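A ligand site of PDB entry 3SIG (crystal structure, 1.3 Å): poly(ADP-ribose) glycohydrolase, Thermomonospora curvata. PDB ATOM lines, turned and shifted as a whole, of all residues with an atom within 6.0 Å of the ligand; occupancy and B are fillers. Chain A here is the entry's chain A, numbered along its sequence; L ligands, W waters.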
ATOM      1  N   GLU A  72     -19.196 -23.788  40.312  1.00  0.00           N
ATOM      2  CA  GLU A  72     -17.761 -23.653  40.256  1.00  0.00           C
ATOM      3  C   GLU A  72     -17.326 -23.115  38.922  1.00  0.00           C
ATOM      4  O   GLU A  72     -17.922 -23.362  37.887  1.00  0.00           O
ATOM      5  CB  GLU A  72     -17.093 -25.018  40.444  1.00  0.00           C
ATOM      6  CG  GLU A  72     -17.247 -25.596  41.823  1.00  0.00           C
ATOM      7  CD  GLU A  72     -16.862 -27.046  41.896  1.00  0.00           C
ATOM      8  OE1 GLU A  72     -17.458 -27.851  41.171  1.00  0.00           O
ATOM      9  OE2 GLU A  72     -15.959 -27.377  42.684  1.00  0.00           O
ATOM     10  N   THR A  73     -16.195 -22.431  38.938  1.00  0.00           N
ATOM     11  CA  THR A  73     -15.455 -22.206  37.714  1.00  0.00           C
ATOM     12  C   THR A  73     -14.898 -23.543  37.210  1.00  0.00           C
ATOM     13  O   THR A  73     -14.764 -24.515  37.959  1.00  0.00           O
ATOM     14  CB  THR A  73     -14.255 -21.275  37.919  1.00  0.00           C
ATOM     15  OG1 THR A  73     -13.367 -21.914  38.850  1.00  0.00           O
ATOM     16  CG2 THR A  73     -14.678 -19.931  38.474  1.00  0.00           C
ATOM     17  N   THR A  74     -14.548 -23.565  35.938  1.00  0.00           N
ATOM     18  CA  THR A  74     -13.874 -24.735  35.342  1.00  0.00           C
ATOM     19  C   THR A  74     -12.687 -25.154  36.207  1.00  0.00           C
ATOM     20  O   THR A  74     -12.523 -26.329  36.552  1.00  0.00           O
ATOM     21  CB  THR A  74     -13.407 -24.433  33.935  1.00  0.00           C
ATOM     22  OG1 THR A  74     -14.507 -23.874  33.179  1.00  0.00           O
ATOM     23  CG2 THR A  74     -12.861 -25.685  33.230  1.00  0.00           C
ATOM     24  N   LEU A  75     -11.827 -24.212  36.516  1.00  0.00           N
ATOM     25  CA  LEU A  75     -10.626 -24.551  37.276  1.00  0.00           C
ATOM     26  C   LEU A  75     -10.907 -24.983  38.687  1.00  0.00           C
ATOM     27  O   LEU A  75     -10.226 -25.886  39.194  1.00  0.00           O
ATOM     28  CB  LEU A  75      -9.657 -23.390  37.249  1.00  0.00           C
ATOM     29  CG  LEU A  75      -9.015 -23.203  35.882  1.00  0.00           C
ATOM     30  CD1 LEU A  75      -8.083 -22.032  35.934  1.00  0.00           C
ATOM     31  CD2 LEU A  75      -8.277 -24.430  35.351  1.00  0.00           C
ATOM     32  N   PHE A  94     -13.611 -23.462  26.373  1.00  0.00           N
ATOM     33  CA  PHE A  94     -14.642 -22.888  25.517  1.00  0.00           C
ATOM     34  C   PHE A  94     -13.916 -21.940  24.551  1.00  0.00           C
ATOM     35  O   PHE A  94     -13.824 -20.705  24.726  1.00  0.00           O
ATOM     36  CB  PHE A  94     -15.674 -22.114  26.342  1.00  0.00           C
ATOM     37  CG  PHE A  94     -16.333 -22.905  27.457  1.00  0.00           C
ATOM     38  CD1 PHE A  94     -16.339 -24.296  27.511  1.00  0.00           C
ATOM     39  CD2 PHE A  94     -17.034 -22.219  28.449  1.00  0.00           C
ATOM     40  CE1 PHE A  94     -16.983 -24.967  28.544  1.00  0.00           C
ATOM     41  CE2 PHE A  94     -17.675 -22.896  29.490  1.00  0.00           C
ATOM     42  CZ  PHE A  94     -17.638 -24.260  29.544  1.00  0.00           C
ATOM     43  N   ALA A  95     -13.367 -22.544  23.515  1.00  0.00           N
ATOM     44  CA  ALA A  95     -12.283 -21.952  22.761  1.00  0.00           C
ATOM     45  C   ALA A  95     -12.707 -20.912  21.757  1.00  0.00           C
ATOM     46  O   ALA A  95     -13.765 -21.026  21.122  1.00  0.00           O
ATOM     47  CB  ALA A  95     -11.587 -23.045  22.032  1.00  0.00           C
ATOM     48  N   SER A  96     -11.806 -19.949  21.533  1.00  0.00           N
ATOM     49  CA  SER A  96     -11.762 -19.150  20.332  1.00  0.00           C
ATOM     50  C   SER A  96     -11.280 -20.037  19.195  1.00  0.00           C
ATOM     51  O   SER A  96     -10.322 -20.809  19.314  1.00  0.00           O
ATOM     52  CB  SER A  96     -10.776 -18.019  20.510  1.00  0.00           C
ATOM     53  OG  SER A  96     -10.580 -17.335  19.261  1.00  0.00           O
ATOM     54  N   ALA A  97     -11.890 -19.893  18.026  1.00  0.00           N
ATOM     55  CA  ALA A  97     -11.409 -20.554  16.825  1.00  0.00           C
ATOM     56  C   ALA A  97     -10.199 -19.866  16.213  1.00  0.00           C
ATOM     57  O   ALA A  97      -9.513 -20.458  15.363  1.00  0.00           O
ATOM     58  CB  ALA A  97     -12.539 -20.611  15.802  1.00  0.00           C
ATOM     59  N   HIS A  99      -7.854 -17.278  18.020  1.00  0.00           N
ATOM     60  CA  HIS A  99      -6.739 -16.813  18.834  1.00  0.00           C
ATOM     61  C   HIS A  99      -6.512 -17.709  20.027  1.00  0.00           C
ATOM     62  O   HIS A  99      -7.428 -17.935  20.808  1.00  0.00           O
ATOM     63  CB  HIS A  99      -6.982 -15.381  19.326  1.00  0.00           C
ATOM     64  CG  HIS A  99      -7.222 -14.405  18.219  1.00  0.00           C
ATOM     65  ND1 HIS A  99      -8.475 -13.930  17.905  1.00  0.00           N
ATOM     66  CD2 HIS A  99      -6.375 -13.872  17.313  1.00  0.00           C
ATOM     67  CE1 HIS A  99      -8.382 -13.115  16.876  1.00  0.00           C
ATOM     68  NE2 HIS A  99      -7.122 -13.060  16.488  1.00  0.00           N
ATOM     69  N   GLY A 101      -5.891 -18.814  23.563  1.00  0.00           N
ATOM     70  CA  GLY A 101      -6.108 -18.073  24.798  1.00  0.00           C
ATOM     71  C   GLY A 101      -7.058 -16.878  24.615  1.00  0.00           C
ATOM     72  O   GLY A 101      -7.217 -16.057  25.538  1.00  0.00           O
ATOM     73  N   GLY A 102      -7.703 -16.777  23.447  1.00  0.00           N
ATOM     74  CA  GLY A 102      -8.664 -15.735  23.217  1.00  0.00           C
ATOM     75  C   GLY A 102      -8.034 -14.371  23.343  1.00  0.00           C
ATOM     76  O   GLY A 102      -6.959 -14.114  22.824  1.00  0.00           O
ATOM     77  N   GLY A 103      -8.725 -13.480  24.039  1.00  0.00           N
ATOM     78  CA  GLY A 103      -8.215 -12.125  24.252  1.00  0.00           C
ATOM     79  C   GLY A 103      -7.425 -11.938  25.556  1.00  0.00           C
ATOM     80  O   GLY A 103      -7.419 -10.853  26.136  1.00  0.00           O
ATOM     81  N   ALA A 108      -9.244  -9.403  28.246  1.00  0.00           N
ATOM     82  CA  ALA A 108     -10.628  -9.833  28.055  1.00  0.00           C
ATOM     83  C   ALA A 108     -11.024 -10.846  29.129  1.00  0.00           C
ATOM     84  O   ALA A 108     -10.174 -11.527  29.701  1.00  0.00           O
ATOM     85  CB  ALA A 108     -10.836 -10.433  26.668  1.00  0.00           C
ATOM     86  N   ALA A 110     -13.505 -13.930  29.839  1.00  0.00           N
ATOM     87  CA  ALA A 110     -14.363 -15.062  29.529  1.00  0.00           C
ATOM     88  C   ALA A 110     -13.609 -16.322  29.975  1.00  0.00           C
ATOM     89  O   ALA A 110     -12.530 -16.232  30.553  1.00  0.00           O
ATOM     90  CB  ALA A 110     -14.731 -15.083  28.047  1.00  0.00           C
ATOM     91  N   GLN A 111     -14.193 -17.489  29.740  1.00  0.00           N
ATOM     92  CA  GLN A 111     -13.642 -18.706  30.308  1.00  0.00           C
ATOM     93  C   GLN A 111     -12.253 -19.041  29.784  1.00  0.00           C
ATOM     94  O   GLN A 111     -11.339 -19.348  30.557  1.00  0.00           O
ATOM     95  CB  GLN A 111     -14.606 -19.889  30.115  1.00  0.00           C
ATOM     96  CG  GLN A 111     -14.213 -21.157  30.832  1.00  0.00           C
ATOM     97  CD  GLN A 111     -13.762 -22.257  29.887  1.00  0.00           C
ATOM     98  OE1 GLN A 111     -13.333 -22.002  28.743  1.00  0.00           O
ATOM     99  NE2 GLN A 111     -13.829 -23.479  30.349  1.00  0.00           N
ATOM    100  N   GLU A 112     -12.049 -18.992  28.484  1.00  0.00           N
ATOM    101  CA  GLU A 112     -10.767 -19.341  27.919  1.00  0.00           C
ATOM    102  C   GLU A 112      -9.677 -18.425  28.456  1.00  0.00           C
ATOM    103  O   GLU A 112      -8.585 -18.861  28.754  1.00  0.00           O
ATOM    104  CB  GLU A 112     -10.780 -19.280  26.379  1.00  0.00           C
ATOM    105  CG  GLU A 112      -9.351 -19.560  25.812  1.00  0.00           C
ATOM    106  CD  GLU A 112      -9.290 -19.781  24.325  1.00  0.00           C
ATOM    107  OE1 GLU A 112     -10.114 -19.189  23.585  1.00  0.00           O
ATOM    108  OE2 GLU A 112      -8.358 -20.513  23.886  1.00  0.00           O
ATOM    109  N   GLU A 113      -9.960 -17.134  28.509  1.00  0.00           N
ATOM    110  CA  GLU A 113      -8.968 -16.181  29.018  1.00  0.00           C
ATOM    111  C   GLU A 113      -8.550 -16.516  30.437  1.00  0.00           C
ATOM    112  O   GLU A 113      -7.388 -16.381  30.793  1.00  0.00           O
ATOM    113  CB  GLU A 113      -9.472 -14.750  28.905  1.00  0.00           C
ATOM    114  CG  GLU A 113      -9.598 -14.242  27.455  1.00  0.00           C
ATOM    115  CD  GLU A 113     -10.881 -14.597  26.727  1.00  0.00           C
ATOM    116  OE1 GLU A 113     -11.720 -15.343  27.257  1.00  0.00           O
ATOM    117  OE2 GLU A 113     -11.037 -14.113  25.588  1.00  0.00           O
ATOM    118  N   ALA A 177     -17.207 -23.821  20.161  1.00  0.00           N
ATOM    119  CA  ALA A 177     -18.617 -23.968  19.851  1.00  0.00           C
ATOM    120  C   ALA A 177     -18.909 -23.090  18.635  1.00  0.00           C
ATOM    121  O   ALA A 177     -18.206 -22.092  18.394  1.00  0.00           O
ATOM    122  CB  ALA A 177     -19.491 -23.543  21.035  1.00  0.00           C
ATOM    123  N   GLY A 218     -19.390 -27.751  30.820  1.00  0.00           N
ATOM    124  CA  GLY A 218     -20.133 -26.568  31.256  1.00  0.00           C
ATOM    125  C   GLY A 218     -20.915 -26.007  30.084  1.00  0.00           C
ATOM    126  O   GLY A 218     -21.187 -26.720  29.102  1.00  0.00           O
ATOM    127  N   ALA A 219     -21.234 -24.724  30.206  1.00  0.00           N
ATOM    128  CA  ALA A 219     -22.107 -24.013  29.285  1.00  0.00           C
ATOM    129  C   ALA A 219     -21.364 -23.493  28.059  1.00  0.00           C
ATOM    130  O   ALA A 219     -21.381 -22.332  27.712  1.00  0.00           O
ATOM    131  CB  ALA A 219     -22.818 -22.889  30.013  1.00  0.00           C
ATOM    132  N   TRP A 220     -20.680 -24.424  27.415  1.00  0.00           N
ATOM    133  CA  TRP A 220     -19.879 -24.259  26.207  1.00  0.00           C
ATOM    134  C   TRP A 220     -20.666 -23.474  25.165  1.00  0.00           C
ATOM    135  O   TRP A 220     -21.820 -23.819  24.855  1.00  0.00           O
ATOM    136  CB  TRP A 220     -19.600 -25.644  25.668  1.00  0.00           C
ATOM    137  CG  TRP A 220     -18.762 -25.780  24.455  1.00  0.00           C
ATOM    138  CD1 TRP A 220     -17.561 -25.176  24.160  1.00  0.00           C
ATOM    139  CD2 TRP A 220     -19.040 -26.683  23.391  1.00  0.00           C
ATOM    140  NE1 TRP A 220     -17.083 -25.659  22.965  1.00  0.00           N
ATOM    141  CE2 TRP A 220     -17.962 -26.596  22.485  1.00  0.00           C
ATOM    142  CE3 TRP A 220     -20.099 -27.576  23.121  1.00  0.00           C
ATOM    143  CZ2 TRP A 220     -17.913 -27.349  21.315  1.00  0.00           C
ATOM    144  CZ3 TRP A 220     -20.054 -28.318  21.959  1.00  0.00           C
ATOM    145  CH2 TRP A 220     -18.980 -28.188  21.067  1.00  0.00           C
ATOM    146  N   GLY A 221     -20.104 -22.378  24.669  1.00  0.00           N
ATOM    147  CA  GLY A 221     -20.740 -21.637  23.608  1.00  0.00           C
ATOM    148  C   GLY A 221     -21.827 -20.672  24.043  1.00  0.00           C
ATOM    149  O   GLY A 221     -22.362 -19.973  23.174  1.00  0.00           O
ATOM    150  N   CYS A 222     -22.163 -20.611  25.320  1.00  0.00           N
ATOM    151  CA  CYS A 222     -23.385 -19.945  25.755  1.00  0.00           C
ATOM    152  C   CYS A 222     -23.221 -18.550  26.308  1.00  0.00           C
ATOM    153  O   CYS A 222     -24.189 -17.991  26.843  1.00  0.00           O
ATOM    154  CB  CYS A 222     -24.122 -20.806  26.785  1.00  0.00           C
ATOM    155  SG  CYS A 222     -24.676 -22.397  26.201  1.00  0.00           S
ATOM    156  N   GLY A 223     -22.009 -17.999  26.196  1.00  0.00           N
ATOM    157  CA  GLY A 223     -21.747 -16.639  26.622  1.00  0.00           C
ATOM    158  C   GLY A 223     -21.389 -15.787  25.433  1.00  0.00           C
ATOM    159  O   GLY A 223     -22.278 -15.347  24.678  1.00  0.00           O
ATOM    160  N   VAL A 224     -20.099 -15.611  25.212  1.00  0.00           N
ATOM    161  CA  VAL A 224     -19.643 -14.808  24.081  1.00  0.00           C
ATOM    162  C   VAL A 224     -20.206 -15.317  22.765  1.00  0.00           C
ATOM    163  O   VAL A 224     -20.538 -14.517  21.893  1.00  0.00           O
ATOM    164  CB  VAL A 224     -18.105 -14.771  24.053  1.00  0.00           C
ATOM    165  CG1 VAL A 224     -17.569 -14.094  22.810  1.00  0.00           C
ATOM    166  CG2 VAL A 224     -17.535 -14.082  25.324  1.00  0.00           C
ATOM    167  N   PHE A 225     -20.316 -16.630  22.601  1.00  0.00           N
ATOM    168  CA  PHE A 225     -20.832 -17.197  21.343  1.00  0.00           C
ATOM    169  C   PHE A 225     -22.361 -17.329  21.241  1.00  0.00           C
ATOM    170  O   PHE A 225     -22.869 -17.714  20.205  1.00  0.00           O
ATOM    171  CB  PHE A 225     -20.172 -18.535  21.079  1.00  0.00           C
ATOM    172  CG  PHE A 225     -18.730 -18.468  20.608  1.00  0.00           C
ATOM    173  CD1 PHE A 225     -18.102 -17.252  20.326  1.00  0.00           C
ATOM    174  CD2 PHE A 225     -18.022 -19.621  20.444  1.00  0.00           C
ATOM    175  CE1 PHE A 225     -16.770 -17.241  19.899  1.00  0.00           C
ATOM    176  CE2 PHE A 225     -16.717 -19.624  19.995  1.00  0.00           C
ATOM    177  CZ  PHE A 225     -16.089 -18.427  19.702  1.00  0.00           C
ATOM    178  N   GLY A 226     -23.088 -16.980  22.281  1.00  0.00           N
ATOM    179  CA  GLY A 226     -24.518 -16.761  22.151  1.00  0.00           C
ATOM    180  C   GLY A 226     -25.374 -17.986  21.896  1.00  0.00           C
ATOM    181  O   GLY A 226     -26.487 -17.853  21.397  1.00  0.00           O
ATOM    182  N   ASN A 227     -24.895 -19.167  22.221  1.00  0.00           N
ATOM    183  CA  ASN A 227     -25.740 -20.351  22.118  1.00  0.00           C
ATOM    184  C   ASN A 227     -26.788 -20.411  23.222  1.00  0.00           C
ATOM    185  O   ASN A 227     -26.659 -19.795  24.273  1.00  0.00           O
ATOM    186  CB  ASN A 227     -24.909 -21.651  22.115  1.00  0.00           C
ATOM    187  CG  ASN A 227     -24.200 -21.884  20.798  1.00  0.00           C
ATOM    188  OD1 ASN A 227     -24.810 -22.415  19.872  1.00  0.00           O
ATOM    189  ND2 ASN A 227     -22.968 -21.445  20.675  1.00  0.00           N
ATOM    190  N   ALA A 256     -19.573 -27.469  35.472  1.00  0.00           N
ATOM    191  CA  ALA A 256     -19.151 -26.365  36.322  1.00  0.00           C
ATOM    192  C   ALA A 256     -19.545 -25.080  35.591  1.00  0.00           C
ATOM    193  O   ALA A 256     -18.963 -24.763  34.548  1.00  0.00           O
ATOM    194  CB  ALA A 256     -17.652 -26.409  36.551  1.00  0.00           C
ATOM    195  N   VAL A 257     -20.590 -24.412  36.095  1.00  0.00           N
ATOM    196  CA  VAL A 257     -21.163 -23.293  35.383  1.00  0.00           C
ATOM    197  C   VAL A 257     -21.138 -22.079  36.306  1.00  0.00           C
ATOM    198  O   VAL A 257     -21.984 -21.943  37.195  1.00  0.00           O
ATOM    199  CB  VAL A 257     -22.572 -23.578  34.910  1.00  0.00           C
ATOM    200  CG1 VAL A 257     -23.008 -22.407  34.009  1.00  0.00           C
ATOM    201  CG2 VAL A 257     -22.642 -24.916  34.150  1.00  0.00           C
ATOM    202  N   TRP A 258     -20.180 -21.171  36.090  1.00  0.00           N
ATOM    203  CA  TRP A 258     -19.973 -19.960  36.849  1.00  0.00           C
ATOM    204  C   TRP A 258     -20.505 -18.808  35.997  1.00  0.00           C
ATOM    205  O   TRP A 258     -19.847 -18.389  35.020  1.00  0.00           O
ATOM    206  CB  TRP A 258     -18.486 -19.766  37.122  1.00  0.00           C
ATOM    207  CG  TRP A 258     -18.201 -18.518  37.897  1.00  0.00           C
ATOM    208  CD1 TRP A 258     -18.706 -18.207  39.113  1.00  0.00           C
ATOM    209  CD2 TRP A 258     -17.452 -17.390  37.473  1.00  0.00           C
ATOM    210  NE1 TRP A 258     -18.282 -16.950  39.506  1.00  0.00           N
ATOM    211  CE2 TRP A 258     -17.501 -16.430  38.506  1.00  0.00           C
ATOM    212  CE3 TRP A 258     -16.702 -17.100  36.342  1.00  0.00           C
ATOM    213  CZ2 TRP A 258     -16.828 -15.199  38.433  1.00  0.00           C
ATOM    214  CZ3 TRP A 258     -16.033 -15.877  36.265  1.00  0.00           C
ATOM    215  CH2 TRP A 258     -16.109 -14.943  37.306  1.00  0.00           C
ATOM    216  N   ASP A 259     -21.689 -18.324  36.362  1.00  0.00           N
ATOM    217  CA  ASP A 259     -22.421 -17.372  35.552  1.00  0.00           C
ATOM    218  C   ASP A 259     -22.743 -16.174  36.446  1.00  0.00           C
ATOM    219  O   ASP A 259     -23.646 -16.245  37.298  1.00  0.00           O
ATOM    220  CB  ASP A 259     -23.719 -17.989  35.031  1.00  0.00           C
ATOM    221  CG  ASP A 259     -24.451 -17.086  34.072  1.00  0.00           C
ATOM    222  OD1 ASP A 259     -24.031 -15.926  33.869  1.00  0.00           O
ATOM    223  OD2 ASP A 259     -25.465 -17.565  33.503  1.00  0.00           O
ATOM    224  N   THR A 260     -22.059 -15.063  36.240  1.00  0.00           N
ATOM    225  CA  THR A 260     -22.236 -13.902  37.073  1.00  0.00           C
ATOM    226  C   THR A 260     -23.399 -13.005  36.652  1.00  0.00           C
ATOM    227  O   THR A 260     -23.678 -12.012  37.318  1.00  0.00           O
ATOM    228  CB  THR A 260     -20.972 -13.041  37.130  1.00  0.00           C
ATOM    229  OG1 THR A 260     -20.604 -12.642  35.813  1.00  0.00           O
ATOM    230  CG2 THR A 260     -19.836 -13.834  37.775  1.00  0.00           C
ATOM    231  N   ARG A 266     -27.308 -19.578  32.614  1.00  0.00           N
ATOM    232  CA  ARG A 266     -26.604 -20.720  32.060  1.00  0.00           C
ATOM    233  C   ARG A 266     -26.586 -21.840  33.092  1.00  0.00           C
ATOM    234  O   ARG A 266     -26.735 -23.024  32.738  1.00  0.00           O
ATOM    235  CB  ARG A 266     -25.163 -20.352  31.640  1.00  0.00           C
ATOM    236  CG  ARG A 266     -25.024 -19.840  30.205  1.00  0.00           C
ATOM    237  CD  ARG A 266     -25.693 -18.537  29.873  1.00  0.00           C
ATOM    238  NE  ARG A 266     -25.269 -17.396  30.683  1.00  0.00           N
ATOM    239  CZ  ARG A 266     -24.911 -16.209  30.215  1.00  0.00           C
ATOM    240  NH1 ARG A 266     -24.797 -15.999  28.919  1.00  0.00           N
ATOM    241  NH2 ARG A 266     -24.633 -15.218  31.053  1.00  0.00           N
ATOM    242  N   HIS A 267     -26.353 -21.488  34.354  1.00  0.00           N
ATOM    243  CA  HIS A 267     -26.317 -22.458  35.405  1.00  0.00           C
ATOM    244  C   HIS A 267     -27.691 -23.051  35.588  1.00  0.00           C
ATOM    245  O   HIS A 267     -27.832 -24.267  35.731  1.00  0.00           O
ATOM    246  CB  HIS A 267     -25.789 -21.858  36.713  1.00  0.00           C
ATOM    247  CG  HIS A 267     -25.922 -22.796  37.867  1.00  0.00           C
ATOM    248  ND1 HIS A 267     -27.055 -22.856  38.653  1.00  0.00           N
ATOM    249  CD2 HIS A 267     -25.087 -23.748  38.362  1.00  0.00           C
ATOM    250  CE1 HIS A 267     -26.920 -23.798  39.563  1.00  0.00           C
ATOM    251  NE2 HIS A 267     -25.729 -24.355  39.407  1.00  0.00           N
HETATM  252  N1  LIG L   1     -15.969 -21.372  34.551  1.00  0.00           N
HETATM  253  C1  LIG L   1     -17.143 -21.929  34.297  1.00  0.00           C
HETATM  254  N2  LIG L   1     -18.170 -21.367  33.589  1.00  0.00           N
HETATM  255  C2  LIG L   1     -17.875 -20.127  33.126  1.00  0.00           C
HETATM  256  C3  LIG L   1     -16.612 -19.478  33.365  1.00  0.00           C
HETATM  257  C4  LIG L   1     -15.690 -20.178  34.105  1.00  0.00           C
HETATM  258  N3  LIG L   1     -14.460 -19.599  34.388  1.00  0.00           N
HETATM  259  N4  LIG L   1     -16.685 -18.213  32.700  1.00  0.00           N
HETATM  260  C5  LIG L   1     -17.872 -18.127  32.176  1.00  0.00           C
HETATM  261  N5  LIG L   1     -18.646 -19.230  32.384  1.00  0.00           N
HETATM  262  P1  LIG L   1     -17.779 -18.184  27.516  1.00  0.00           P
HETATM  263  P2  LIG L   1     -18.251 -19.193  24.750  1.00  0.00           P
HETATM  264  C6  LIG L   1     -20.001 -19.571  31.956  1.00  0.00           C
HETATM  265  O1  LIG L   1     -18.594 -16.988  27.189  1.00  0.00           O
HETATM  266  O2  LIG L   1     -17.938 -20.580  24.234  1.00  0.00           O
HETATM  267  C7  LIG L   1     -13.746 -16.294  24.723  1.00  0.00           C
HETATM  268  O3  LIG L   1     -13.323 -14.989  24.444  1.00  0.00           O
HETATM  269  C8  LIG L   1     -20.894 -18.377  31.703  1.00  0.00           C
HETATM  270  O4  LIG L   1     -22.205 -18.680  32.065  1.00  0.00           O
HETATM  271  O5  LIG L   1     -16.369 -17.981  28.015  1.00  0.00           O
HETATM  272  O6  LIG L   1     -19.669 -18.729  24.706  1.00  0.00           O
HETATM  273  C9  LIG L   1     -13.077 -17.191  23.766  1.00  0.00           C
HETATM  274  O7  LIG L   1     -11.709 -17.021  23.586  1.00  0.00           O
HETATM  275  C10 LIG L   1     -20.784 -18.212  30.226  1.00  0.00           C
HETATM  276  O8  LIG L   1     -21.930 -17.650  29.670  1.00  0.00           O
HETATM  277  O9  LIG L   1     -17.772 -19.183  26.271  1.00  0.00           O
HETATM  278  C11 LIG L   1     -14.001 -17.307  22.635  1.00  0.00           C
HETATM  279  O10 LIG L   1     -13.642 -16.254  21.778  1.00  0.00           O
HETATM  280  C12 LIG L   1     -20.569 -19.607  29.705  1.00  0.00           C
HETATM  281  O11 LIG L   1     -20.009 -20.338  30.774  1.00  0.00           O
HETATM  282  C13 LIG L   1     -15.329 -17.112  23.286  1.00  0.00           C
HETATM  283  O12 LIG L   1     -15.133 -16.389  24.495  1.00  0.00           O
HETATM  284  C14 LIG L   1     -19.690 -19.719  28.467  1.00  0.00           C
HETATM  285  O13 LIG L   1     -18.445 -19.085  28.680  1.00  0.00           O
HETATM  286  C15 LIG L   1     -16.077 -18.422  23.571  1.00  0.00           C
HETATM  287  O14 LIG L   1     -17.367 -18.093  24.043  1.00  0.00           O
HETATM  288  O   HOH W   1     -11.817 -12.034  23.797  1.00  0.00           O
HETATM  289  O   HOH W   2     -12.887 -17.112  33.883  1.00  0.00           O
HETATM  290  O   HOH W   3     -11.299 -14.387  22.126  1.00  0.00           O
HETATM  291  O   HOH W   4     -11.986 -21.277  35.470  1.00  0.00           O
HETATM  292  O   HOH W   5     -14.166 -18.746  26.639  1.00  0.00           O
HETATM  293  O   HOH W   6     -14.493 -12.456  24.451  1.00  0.00           O
HETATM  294  O   HOH W   7     -21.479 -15.016  29.835  1.00  0.00           O
HETATM  295  O   HOH W   8     -13.717 -15.577  19.248  1.00  0.00           O
HETATM  296  O   HOH W   9     -16.376 -22.136  22.459  1.00  0.00           O
HETATM  297  O   HOH W  10     -18.944 -14.908  28.800  1.00  0.00           O
HETATM  298  O   HOH W  11     -11.459 -19.573  33.330  1.00  0.00           O
HETATM  299  O   HOH W  12     -19.773 -23.428  32.272  1.00  0.00           O
HETATM  300  O   HOH W  13     -15.081 -15.903  32.795  1.00  0.00           O
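The backbone NH (N) of Thr 74 lies within hydrogen-bond range of a nitrogen (N1) of the ligand, 3.0 Å away. The backbone NH of Gly 221 lies within hydrogen-bond range of an oxygen (O2) of the ligand, 2.8 Å away. The backbone NH (N) of Cys 222 lies within hydrogen-bond range of an oxygen (O6) of the ligand, 3.2 Å away. OE1 of Glu 112 sits at hydrogen-bond distance from O7 of the ligand, 2.7 Å away. The side-chain hydroxyl (OG1) of Thr 74 is in hydrogen-bond range of a nitrogen (N1) of the ligand. O6 of the ligand is in hydrogen-bond range of N of Gly 223, at 2.9 Å. O3 of the ligand is in hydrogen-bond range of OE2 of Glu 113 (2.7 Å). The backbone NH (N) of Trp 258 lies within hydrogen-bond range of a nitrogen (N2) of the ligand (3.2 Å). An oxygen (O6) of the ligand is in hydrogen-bond range of the backbone NH (N) of Phe 225, at 3.0 Å. The backbone NH of Gln 111 lies within hydrogen-bond range of an oxygen (O5) of the ligand. N of Val 224 lies within hydrogen-bond range of O1 of the ligand, at 2.8 Å. O8 of the ligand sits close to NH1 of Arg 266, 3.4 Å away.
The backbone NH (N) of Gly 101 is in hydrogen-bond range of the side-chain carboxylate (OE2) of Glu 112. The backbone NH of His 99 is in hydrogen-bond range of the side-chain hydroxyl of Ser 96 (3.0 Å). The backbone carbonyl oxygen (O) of Cys 222 sits at hydrogen-bond distance from the guanidinium group (NH1) of Arg 266, at 2.9 Å. OE1 of Glu 112 lies within hydrogen-bond range of N of Ser 96 (2.8 Å). The side-chain sulfur (SG) of Cys 222 sits at hydrogen-bond distance from the backbone carbonyl oxygen (O) of Trp 220, at 3.5 Å. N of Val 257 lies within hydrogen-bond range of O of Glu 72. OE1 of Gln 111 lies within hydrogen-bond range of N of Phe 94 (2.8 Å). N of Ala 110 sits close to OE1 of Glu 113 (3.4 Å).
O of Glu 72 touches C1 of the ligand, at 3.9 Å. Thr 73 touches the ligand (CA to N1, 3.3 Å). O of Phe 94 touches C15 of the ligand, 3.4 Å away. C of Ala 95 touches C11 of the ligand (3.9 Å). Ser 96 touches the ligand. Gly 102 touches the ligand. CB of Ala 110 touches O5 of the ligand, at 3.3 Å. O of Ala 219 touches C14 of the ligand, at 3.2 Å. Ala 256 touches the ligand (O to C1, 3.4 Å). Val 257 touches the ligand (CA to N2, 3.99 Å). Asp 259 touches the ligand. Hydrophobic or aromatic side chains within 4 Å of the ligand: Phe 94, Ala 110, Ala 219, Val 224, Phe 225 and Trp 258. Along chain A the residues within 4 Å of the ligand span positions 72 to 266. The nearest printed residue that does not touch the ligand is Trp 220 (4.1 Å).
Water W7 lies within hydrogen-bond range of O8 of the ligand (2.7 Å) and NH2 of Arg 266 (3.4 Å). Water W9 lies within hydrogen-bond range of an oxygen (O2) of the ligand (2.8 Å), the backbone NH of Ala 177 (3.0 Å) and the backbone carbonyl oxygen of Ala 95 (3.1 Å). Water W12 lies within hydrogen-bond range of O of Ala 256 (2.8 Å), N of Ala 219 (2.8 Å) and N2 of the ligand (2.9 Å). Water W2 bridges a nitrogen (N3) of the ligand (3.0 Å) and the backbone carbonyl oxygen of Ala 110 (3.5 Å). Water W3 lies within hydrogen-bond range of O10 of the ligand (3.0 Å), N of Gly 103 (3.3 Å) and OE2 of Glu 113 (3.5 Å). Water W1 lies within hydrogen-bond range of OE2 of Glu 113 (2.9 Å), O3 of the ligand (3.4 Å) and N of Gly 103 (3.4 Å).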
